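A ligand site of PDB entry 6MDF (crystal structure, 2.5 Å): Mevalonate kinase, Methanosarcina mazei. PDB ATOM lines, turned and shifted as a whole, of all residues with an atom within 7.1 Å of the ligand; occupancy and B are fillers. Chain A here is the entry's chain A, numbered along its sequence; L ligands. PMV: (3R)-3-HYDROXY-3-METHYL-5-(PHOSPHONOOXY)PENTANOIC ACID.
NE2 of His 18 lies within hydrogen-bond range of O of Ala 261, at 2.6 Å. The side-chain amino group (NZ) of Lys 11 is in salt-bridge range of the side-chain carboxylate (OD1) of Asp 140 (2.7 Å). The backbone carbonyl oxygen (O) of Gly 93 lies within hydrogen-bond range of the side-chain hydroxyl (OG1) of Thr 259. The backbone NH (N) of Gly 260 lies within hydrogen-bond range of the side-chain carboxylate (OE2) of Glu 17 (3.1 Å). The side-chain hydroxyl of Ser 92 sits at hydrogen-bond distance from the backbone carbonyl oxygen of Thr 259 (3.3 Å). OG1 of Thr 259 sits at hydrogen-bond distance from N of Tyr 13, 3.1 Å away. The backbone carbonyl oxygen (O) of Leu 94 sits at hydrogen-bond distance from the backbone NH (N) of Lys 11 (3.0 Å).
CE2 of Tyr 13 touches O5 of the ligand, 3.9 Å away. Glu 17 touches the ligand (C to O3A, 3.9 Å). Val 21 touches the ligand. Ser 92 touches the ligand (O to OP2, 3.7 Å). CA of Gly 93 touches OP2 of the ligand, 3.2 Å away. CG2 of Thr 176 touches C3A of the ligand (3.6 Å). CG2 of Val 180 touches C3A of the ligand, at 3.7 Å. Gly 260 touches the ligand. Ala 261 touches the ligand (N to C5, 3.6 Å). Of the 31 residues printed, 12 come within 4 Å of the ligand.
The backbone NH (N) of His 18 is in hydrogen-bond range of an oxygen (O3A) of the ligand (2.8 Å). OD2 of Asp 140 lies close to OP3 of the ligand (3.1 Å). An oxygen (OP3) of the ligand is in salt-bridge range of the side-chain amino group of Lys 11 (3.9 Å).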
ATOM      1  N   LYS A  11       2.154  17.429 -21.950  1.00  0.00           N
ATOM      2  CA  LYS A  11       2.589  18.426 -20.979  1.00  0.00           C
ATOM      3  C   LYS A  11       4.027  18.178 -20.571  1.00  0.00           C
ATOM      4  O   LYS A  11       4.592  17.106 -20.800  1.00  0.00           O
ATOM      5  CB  LYS A  11       1.679  18.421 -19.746  1.00  0.00           C
ATOM      6  CG  LYS A  11       2.026  17.339 -18.741  1.00  0.00           C
ATOM      7  CD  LYS A  11       0.858  17.032 -17.817  1.00  0.00           C
ATOM      8  CE  LYS A  11       1.209  15.916 -16.844  1.00  0.00           C
ATOM      9  NZ  LYS A  11       1.661  14.670 -17.533  1.00  0.00           N
ATOM     10  N   TYR A  13       6.721  19.140 -17.062  1.00  0.00           N
ATOM     11  CA  TYR A  13       6.791  19.624 -15.695  1.00  0.00           C
ATOM     12  C   TYR A  13       7.759  20.793 -15.624  1.00  0.00           C
ATOM     13  O   TYR A  13       8.959  20.639 -15.879  1.00  0.00           O
ATOM     14  CB  TYR A  13       7.253  18.506 -14.746  1.00  0.00           C
ATOM     15  CG  TYR A  13       6.161  17.551 -14.324  1.00  0.00           C
ATOM     16  CD1 TYR A  13       5.387  17.793 -13.198  1.00  0.00           C
ATOM     17  CD2 TYR A  13       5.913  16.384 -15.044  1.00  0.00           C
ATOM     18  CE1 TYR A  13       4.396  16.911 -12.807  1.00  0.00           C
ATOM     19  CE2 TYR A  13       4.920  15.502 -14.663  1.00  0.00           C
ATOM     20  CZ  TYR A  13       4.164  15.770 -13.540  1.00  0.00           C
ATOM     21  OH  TYR A  13       3.184  14.895 -13.151  1.00  0.00           O
ATOM     22  N   GLY A  16       8.676  20.252  -9.868  1.00  0.00           N
ATOM     23  CA  GLY A  16       7.994  19.494  -8.835  1.00  0.00           C
ATOM     24  C   GLY A  16       7.693  18.037  -9.119  1.00  0.00           C
ATOM     25  O   GLY A  16       6.990  17.411  -8.314  1.00  0.00           O
ATOM     26  N   GLU A  17       8.197  17.479 -10.214  1.00  0.00           N
ATOM     27  CA  GLU A  17       8.004  16.056 -10.440  1.00  0.00           C
ATOM     28  C   GLU A  17       8.706  15.238  -9.352  1.00  0.00           C
ATOM     29  O   GLU A  17       9.631  15.714  -8.683  1.00  0.00           O
ATOM     30  CB  GLU A  17       8.515  15.629 -11.820  1.00  0.00           C
ATOM     31  CG  GLU A  17       9.916  16.113 -12.135  1.00  0.00           C
ATOM     32  CD  GLU A  17       9.925  17.368 -12.979  1.00  0.00           C
ATOM     33  OE1 GLU A  17       9.949  18.470 -12.407  1.00  0.00           O
ATOM     34  OE2 GLU A  17       9.870  17.228 -14.219  1.00  0.00           O
ATOM     35  N   HIS A  18       8.225  14.010  -9.172  1.00  0.00           N
ATOM     36  CA  HIS A  18       8.718  13.062  -8.175  1.00  0.00           C
ATOM     37  C   HIS A  18       8.354  13.478  -6.745  1.00  0.00           C
ATOM     38  O   HIS A  18       8.047  12.622  -5.909  1.00  0.00           O
ATOM     39  CB  HIS A  18      10.231  12.853  -8.294  1.00  0.00           C
ATOM     40  CG  HIS A  18      10.620  11.761  -9.233  1.00  0.00           C
ATOM     41  ND1 HIS A  18      10.538  10.423  -8.887  1.00  0.00           N
ATOM     42  CD2 HIS A  18      11.119  11.802 -10.488  1.00  0.00           C
ATOM     43  CE1 HIS A  18      10.961   9.683  -9.907  1.00  0.00           C
ATOM     44  NE2 HIS A  18      11.318  10.497 -10.888  1.00  0.00           N
ATOM     45  N   ALA A  19       8.384  14.775  -6.456  1.00  0.00           N
ATOM     46  CA  ALA A  19       8.048  15.252  -5.123  1.00  0.00           C
ATOM     47  C   ALA A  19       6.542  15.328  -4.885  1.00  0.00           C
ATOM     48  O   ALA A  19       6.133  15.403  -3.719  1.00  0.00           O
ATOM     49  CB  ALA A  19       8.670  16.634  -4.880  1.00  0.00           C
ATOM     50  N   VAL A  20       5.732  15.303  -5.938  1.00  0.00           N
ATOM     51  CA  VAL A  20       4.281  15.350  -5.753  1.00  0.00           C
ATOM     52  C   VAL A  20       3.790  14.128  -5.008  1.00  0.00           C
ATOM     53  O   VAL A  20       2.927  14.220  -4.122  1.00  0.00           O
ATOM     54  CB  VAL A  20       3.563  15.505  -7.108  1.00  0.00           C
ATOM     55  CG1 VAL A  20       2.172  14.893  -7.054  1.00  0.00           C
ATOM     56  CG2 VAL A  20       3.449  16.952  -7.471  1.00  0.00           C
ATOM     57  N   VAL A  21       4.335  12.953  -5.327  1.00  0.00           N
ATOM     58  CA  VAL A  21       3.910  11.717  -4.699  1.00  0.00           C
ATOM     59  C   VAL A  21       4.143  11.722  -3.194  1.00  0.00           C
ATOM     60  O   VAL A  21       3.665  10.827  -2.495  1.00  0.00           O
ATOM     61  CB  VAL A  21       4.604  10.506  -5.349  1.00  0.00           C
ATOM     62  CG1 VAL A  21       4.632  10.664  -6.866  1.00  0.00           C
ATOM     63  CG2 VAL A  21       6.012  10.335  -4.800  1.00  0.00           C
ATOM     64  N   ALA A  26       3.675  21.079  -7.458  1.00  0.00           N
ATOM     65  CA  ALA A  26       4.335  21.040  -8.750  1.00  0.00           C
ATOM     66  C   ALA A  26       3.567  21.935  -9.709  1.00  0.00           C
ATOM     67  O   ALA A  26       2.445  22.359  -9.424  1.00  0.00           O
ATOM     68  CB  ALA A  26       4.442  19.619  -9.306  1.00  0.00           C
ATOM     69  N   GLY A  91       7.130   7.443 -23.833  1.00  0.00           N
ATOM     70  CA  GLY A  91       8.347   7.494 -23.053  1.00  0.00           C
ATOM     71  C   GLY A  91       8.579   8.887 -22.519  1.00  0.00           C
ATOM     72  O   GLY A  91       8.082   9.864 -23.095  1.00  0.00           O
ATOM     73  N   SER A  92       9.328   8.995 -21.421  1.00  0.00           N
ATOM     74  CA  SER A  92       9.540  10.256 -20.702  1.00  0.00           C
ATOM     75  C   SER A  92       8.243  10.806 -20.130  1.00  0.00           C
ATOM     76  O   SER A  92       7.169  10.236 -20.339  1.00  0.00           O
ATOM     77  CB  SER A  92      10.185  11.301 -21.618  1.00  0.00           C
ATOM     78  OG  SER A  92      10.462  12.491 -20.894  1.00  0.00           O
ATOM     79  N   GLY A  93       8.348  11.901 -19.381  1.00  0.00           N
ATOM     80  CA  GLY A  93       7.181  12.528 -18.806  1.00  0.00           C
ATOM     81  C   GLY A  93       6.597  13.601 -19.709  1.00  0.00           C
ATOM     82  O   GLY A  93       6.677  14.800 -19.402  1.00  0.00           O
ATOM     83  N   LEU A  94       6.013  13.173 -20.830  1.00  0.00           N
ATOM     84  CA  LEU A  94       5.296  14.076 -21.718  1.00  0.00           C
ATOM     85  C   LEU A  94       3.788  13.830 -21.722  1.00  0.00           C
ATOM     86  O   LEU A  94       3.059  14.569 -22.396  1.00  0.00           O
ATOM     87  CB  LEU A  94       5.845  13.981 -23.140  1.00  0.00           C
ATOM     88  CG  LEU A  94       7.316  14.365 -23.339  1.00  0.00           C
ATOM     89  CD1 LEU A  94       7.604  14.606 -24.809  1.00  0.00           C
ATOM     90  CD2 LEU A  94       7.680  15.586 -22.511  1.00  0.00           C
ATOM     91  N   GLY A  95       3.320  12.818 -21.018  1.00  0.00           N
ATOM     92  CA  GLY A  95       1.887  12.543 -20.937  1.00  0.00           C
ATOM     93  C   GLY A  95       1.264  11.985 -22.196  1.00  0.00           C
ATOM     94  O   GLY A  95       0.151  12.391 -22.558  1.00  0.00           O
ATOM     95  N   SER A  96       1.944  11.059 -22.866  1.00  0.00           N
ATOM     96  CA  SER A  96       1.388  10.483 -24.089  1.00  0.00           C
ATOM     97  C   SER A  96       0.201   9.582 -23.779  1.00  0.00           C
ATOM     98  O   SER A  96      -0.781   9.547 -24.538  1.00  0.00           O
ATOM     99  CB  SER A  96       2.458   9.720 -24.861  1.00  0.00           C
ATOM    100  OG  SER A  96       2.728   8.466 -24.252  1.00  0.00           O
ATOM    101  N   SER A  97       0.258   8.840 -22.671  1.00  0.00           N
ATOM    102  CA  SER A  97      -0.837   7.934 -22.330  1.00  0.00           C
ATOM    103  C   SER A  97      -2.075   8.721 -21.909  1.00  0.00           C
ATOM    104  O   SER A  97      -3.207   8.331 -22.234  1.00  0.00           O
ATOM    105  CB  SER A  97      -0.411   6.968 -21.226  1.00  0.00           C
ATOM    106  OG  SER A  97      -0.231   7.634 -19.991  1.00  0.00           O
ATOM    107  N   ALA A  98      -1.899   9.826 -21.186  1.00  0.00           N
ATOM    108  CA  ALA A  98      -3.037  10.655 -20.806  1.00  0.00           C
ATOM    109  C   ALA A  98      -3.635  11.375 -22.011  1.00  0.00           C
ATOM    110  O   ALA A  98      -4.860  11.566 -22.057  1.00  0.00           O
ATOM    111  CB  ALA A  98      -2.639  11.678 -19.744  1.00  0.00           C
ATOM    112  N   GLU A 129      -6.859   5.460 -16.455  1.00  0.00           N
ATOM    113  CA  GLU A 129      -5.455   5.260 -16.121  1.00  0.00           C
ATOM    114  C   GLU A 129      -5.274   4.425 -14.858  1.00  0.00           C
ATOM    115  O   GLU A 129      -4.201   3.837 -14.665  1.00  0.00           O
ATOM    116  CB  GLU A 129      -4.747   6.602 -15.968  1.00  0.00           C
ATOM    117  CG  GLU A 129      -4.327   7.238 -17.285  1.00  0.00           C
ATOM    118  CD  GLU A 129      -3.310   8.345 -17.103  1.00  0.00           C
ATOM    119  OE1 GLU A 129      -3.416   9.095 -16.111  1.00  0.00           O
ATOM    120  OE2 GLU A 129      -2.398   8.459 -17.954  1.00  0.00           O
ATOM    121  N   GLN A 133      -3.064   1.032 -15.150  1.00  0.00           N
ATOM    122  CA  GLN A 133      -1.810   1.060 -14.409  1.00  0.00           C
ATOM    123  C   GLN A 133      -1.941   0.553 -12.979  1.00  0.00           C
ATOM    124  O   GLN A 133      -0.935   0.454 -12.269  1.00  0.00           O
ATOM    125  CB  GLN A 133      -1.239   2.478 -14.400  1.00  0.00           C
ATOM    126  CG  GLN A 133      -1.107   3.091 -15.776  1.00  0.00           C
ATOM    127  CD  GLN A 133      -0.859   4.585 -15.735  1.00  0.00           C
ATOM    128  OE1 GLN A 133      -0.832   5.185 -14.663  1.00  0.00           O
ATOM    129  NE2 GLN A 133      -0.685   5.184 -16.907  1.00  0.00           N
ATOM    130  N   SER A 137      -2.287   8.913 -10.751  1.00  0.00           N
ATOM    131  CA  SER A 137      -2.619  10.241 -10.260  1.00  0.00           C
ATOM    132  C   SER A 137      -3.545  10.951 -11.250  1.00  0.00           C
ATOM    133  O   SER A 137      -3.386  10.791 -12.465  1.00  0.00           O
ATOM    134  CB  SER A 137      -1.358  11.069 -10.045  1.00  0.00           C
ATOM    135  OG  SER A 137      -1.671  12.447  -9.966  1.00  0.00           O
ATOM    136  N   THR A 139      -3.473  13.802 -12.154  1.00  0.00           N
ATOM    137  CA  THR A 139      -2.782  14.986 -12.667  1.00  0.00           C
ATOM    138  C   THR A 139      -2.673  14.954 -14.186  1.00  0.00           C
ATOM    139  O   THR A 139      -2.964  15.949 -14.868  1.00  0.00           O
ATOM    140  CB  THR A 139      -1.405  15.100 -12.023  1.00  0.00           C
ATOM    141  OG1 THR A 139      -1.545  15.582 -10.681  1.00  0.00           O
ATOM    142  CG2 THR A 139      -0.511  16.056 -12.800  1.00  0.00           C
ATOM    143  N   ASP A 140      -2.258  13.818 -14.753  1.00  0.00           N
ATOM    144  CA  ASP A 140      -1.981  13.750 -16.186  1.00  0.00           C
ATOM    145  C   ASP A 140      -3.229  14.019 -17.014  1.00  0.00           C
ATOM    146  O   ASP A 140      -3.217  14.843 -17.929  1.00  0.00           O
ATOM    147  CB  ASP A 140      -1.370  12.398 -16.544  1.00  0.00           C
ATOM    148  CG  ASP A 140      -0.039  12.161 -15.867  1.00  0.00           C
ATOM    149  OD1 ASP A 140       0.638  13.145 -15.512  1.00  0.00           O
ATOM    150  OD2 ASP A 140       0.337  10.974 -15.689  1.00  0.00           O
ATOM    151  N   SER A 174      12.189   5.769 -20.612  1.00  0.00           N
ATOM    152  CA  SER A 174      11.953   6.239 -19.250  1.00  0.00           C
ATOM    153  C   SER A 174      10.870   5.373 -18.624  1.00  0.00           C
ATOM    154  O   SER A 174       9.672   5.579 -18.860  1.00  0.00           O
ATOM    155  CB  SER A 174      11.567   7.719 -19.256  1.00  0.00           C
ATOM    156  OG  SER A 174      11.213   8.158 -17.950  1.00  0.00           O
ATOM    157  N   THR A 176       8.810   4.731 -15.753  1.00  0.00           N
ATOM    158  CA  THR A 176       8.429   5.557 -14.617  1.00  0.00           C
ATOM    159  C   THR A 176       8.402   4.753 -13.319  1.00  0.00           C
ATOM    160  O   THR A 176       8.894   5.225 -12.289  1.00  0.00           O
ATOM    161  CB  THR A 176       7.057   6.199 -14.877  1.00  0.00           C
ATOM    162  OG1 THR A 176       7.162   7.113 -15.975  1.00  0.00           O
ATOM    163  CG2 THR A 176       6.551   6.930 -13.644  1.00  0.00           C
ATOM    164  N   LYS A 177       7.838   3.551 -13.356  1.00  0.00           N
ATOM    165  CA  LYS A 177       7.568   2.805 -12.126  1.00  0.00           C
ATOM    166  C   LYS A 177       8.845   2.525 -11.346  1.00  0.00           C
ATOM    167  O   LYS A 177       8.887   2.710 -10.123  1.00  0.00           O
ATOM    168  CB  LYS A 177       6.835   1.505 -12.446  1.00  0.00           C
ATOM    169  N   LEU A 179      11.790   4.083 -11.564  1.00  0.00           N
ATOM    170  CA  LEU A 179      12.428   5.313 -11.093  1.00  0.00           C
ATOM    171  C   LEU A 179      11.727   5.852  -9.853  1.00  0.00           C
ATOM    172  O   LEU A 179      12.385   6.344  -8.920  1.00  0.00           O
ATOM    173  CB  LEU A 179      12.440   6.358 -12.208  1.00  0.00           C
ATOM    174  CG  LEU A 179      13.397   6.020 -13.346  1.00  0.00           C
ATOM    175  CD1 LEU A 179      12.999   6.772 -14.604  1.00  0.00           C
ATOM    176  CD2 LEU A 179      14.830   6.325 -12.945  1.00  0.00           C
ATOM    177  N   VAL A 180      10.392   5.796  -9.819  1.00  0.00           N
ATOM    178  CA  VAL A 180       9.674   6.161  -8.610  1.00  0.00           C
ATOM    179  C   VAL A 180      10.024   5.208  -7.479  1.00  0.00           C
ATOM    180  O   VAL A 180      10.142   5.609  -6.308  1.00  0.00           O
ATOM    181  CB  VAL A 180       8.155   6.210  -8.871  1.00  0.00           C
ATOM    182  CG1 VAL A 180       7.392   6.518  -7.592  1.00  0.00           C
ATOM    183  CG2 VAL A 180       7.837   7.229  -9.946  1.00  0.00           C
ATOM    184  N   THR A 259      12.070  16.510 -17.490  1.00  0.00           N
ATOM    185  CA  THR A 259      10.622  16.545 -17.326  1.00  0.00           C
ATOM    186  C   THR A 259      10.123  15.110 -17.229  1.00  0.00           C
ATOM    187  O   THR A 259      10.301  14.310 -18.166  1.00  0.00           O
ATOM    188  CB  THR A 259       9.938  17.292 -18.471  1.00  0.00           C
ATOM    189  OG1 THR A 259       8.522  17.053 -18.413  1.00  0.00           O
ATOM    190  CG2 THR A 259      10.467  16.841 -19.835  1.00  0.00           C
ATOM    191  N   GLY A 260       9.507  14.775 -16.099  1.00  0.00           N
ATOM    192  CA  GLY A 260       8.977  13.437 -15.891  1.00  0.00           C
ATOM    193  C   GLY A 260       9.807  12.607 -14.934  1.00  0.00           C
ATOM    194  O   GLY A 260      10.531  13.139 -14.097  1.00  0.00           O
ATOM    195  N   ALA A 261       9.726  11.280 -15.079  1.00  0.00           N
ATOM    196  CA  ALA A 261      10.371  10.379 -14.134  1.00  0.00           C
ATOM    197  C   ALA A 261      11.889  10.463 -14.197  1.00  0.00           C
ATOM    198  O   ALA A 261      12.559  10.172 -13.203  1.00  0.00           O
ATOM    199  CB  ALA A 261       9.930   8.933 -14.387  1.00  0.00           C
ATOM    200  N   GLY A 262      12.447  10.857 -15.334  1.00  0.00           N
ATOM    201  CA  GLY A 262      13.883  10.909 -15.482  1.00  0.00           C
ATOM    202  C   GLY A 262      14.464   9.592 -15.976  1.00  0.00           C
ATOM    203  O   GLY A 262      13.808   8.876 -16.740  1.00  0.00           O
HETATM  204  OP2 PMV L   1       5.596  10.432 -16.951  1.00  0.00           O
HETATM  205  P   PMV L   1       4.447  10.611 -15.980  1.00  0.00           P
HETATM  206  OP3 PMV L   1       3.243  11.163 -16.708  1.00  0.00           O
HETATM  207  OP1 PMV L   1       4.104   9.267 -15.362  1.00  0.00           O
HETATM  208  O5  PMV L   1       4.893  11.646 -14.774  1.00  0.00           O
HETATM  209  C5  PMV L   1       6.210  11.582 -14.295  1.00  0.00           C
HETATM  210  C4  PMV L   1       6.330  12.332 -12.963  1.00  0.00           C
HETATM  211  C3  PMV L   1       6.323  11.361 -11.785  1.00  0.00           C
HETATM  212  O3A PMV L   1       6.903  12.010 -10.649  1.00  0.00           O
HETATM  213  C3A PMV L   1       7.173  10.139 -12.111  1.00  0.00           C
HETATM  214  C2  PMV L   1       4.900  10.915 -11.475  1.00  0.00           C
HETATM  215  C1  PMV L   1       4.302  11.784 -10.363  1.00  0.00           C
HETATM  216  O2  PMV L   1       3.269  11.382  -9.757  1.00  0.00           O
HETATM  217  O1  PMV L   1       4.830  12.883 -10.064  1.00  0.00           O
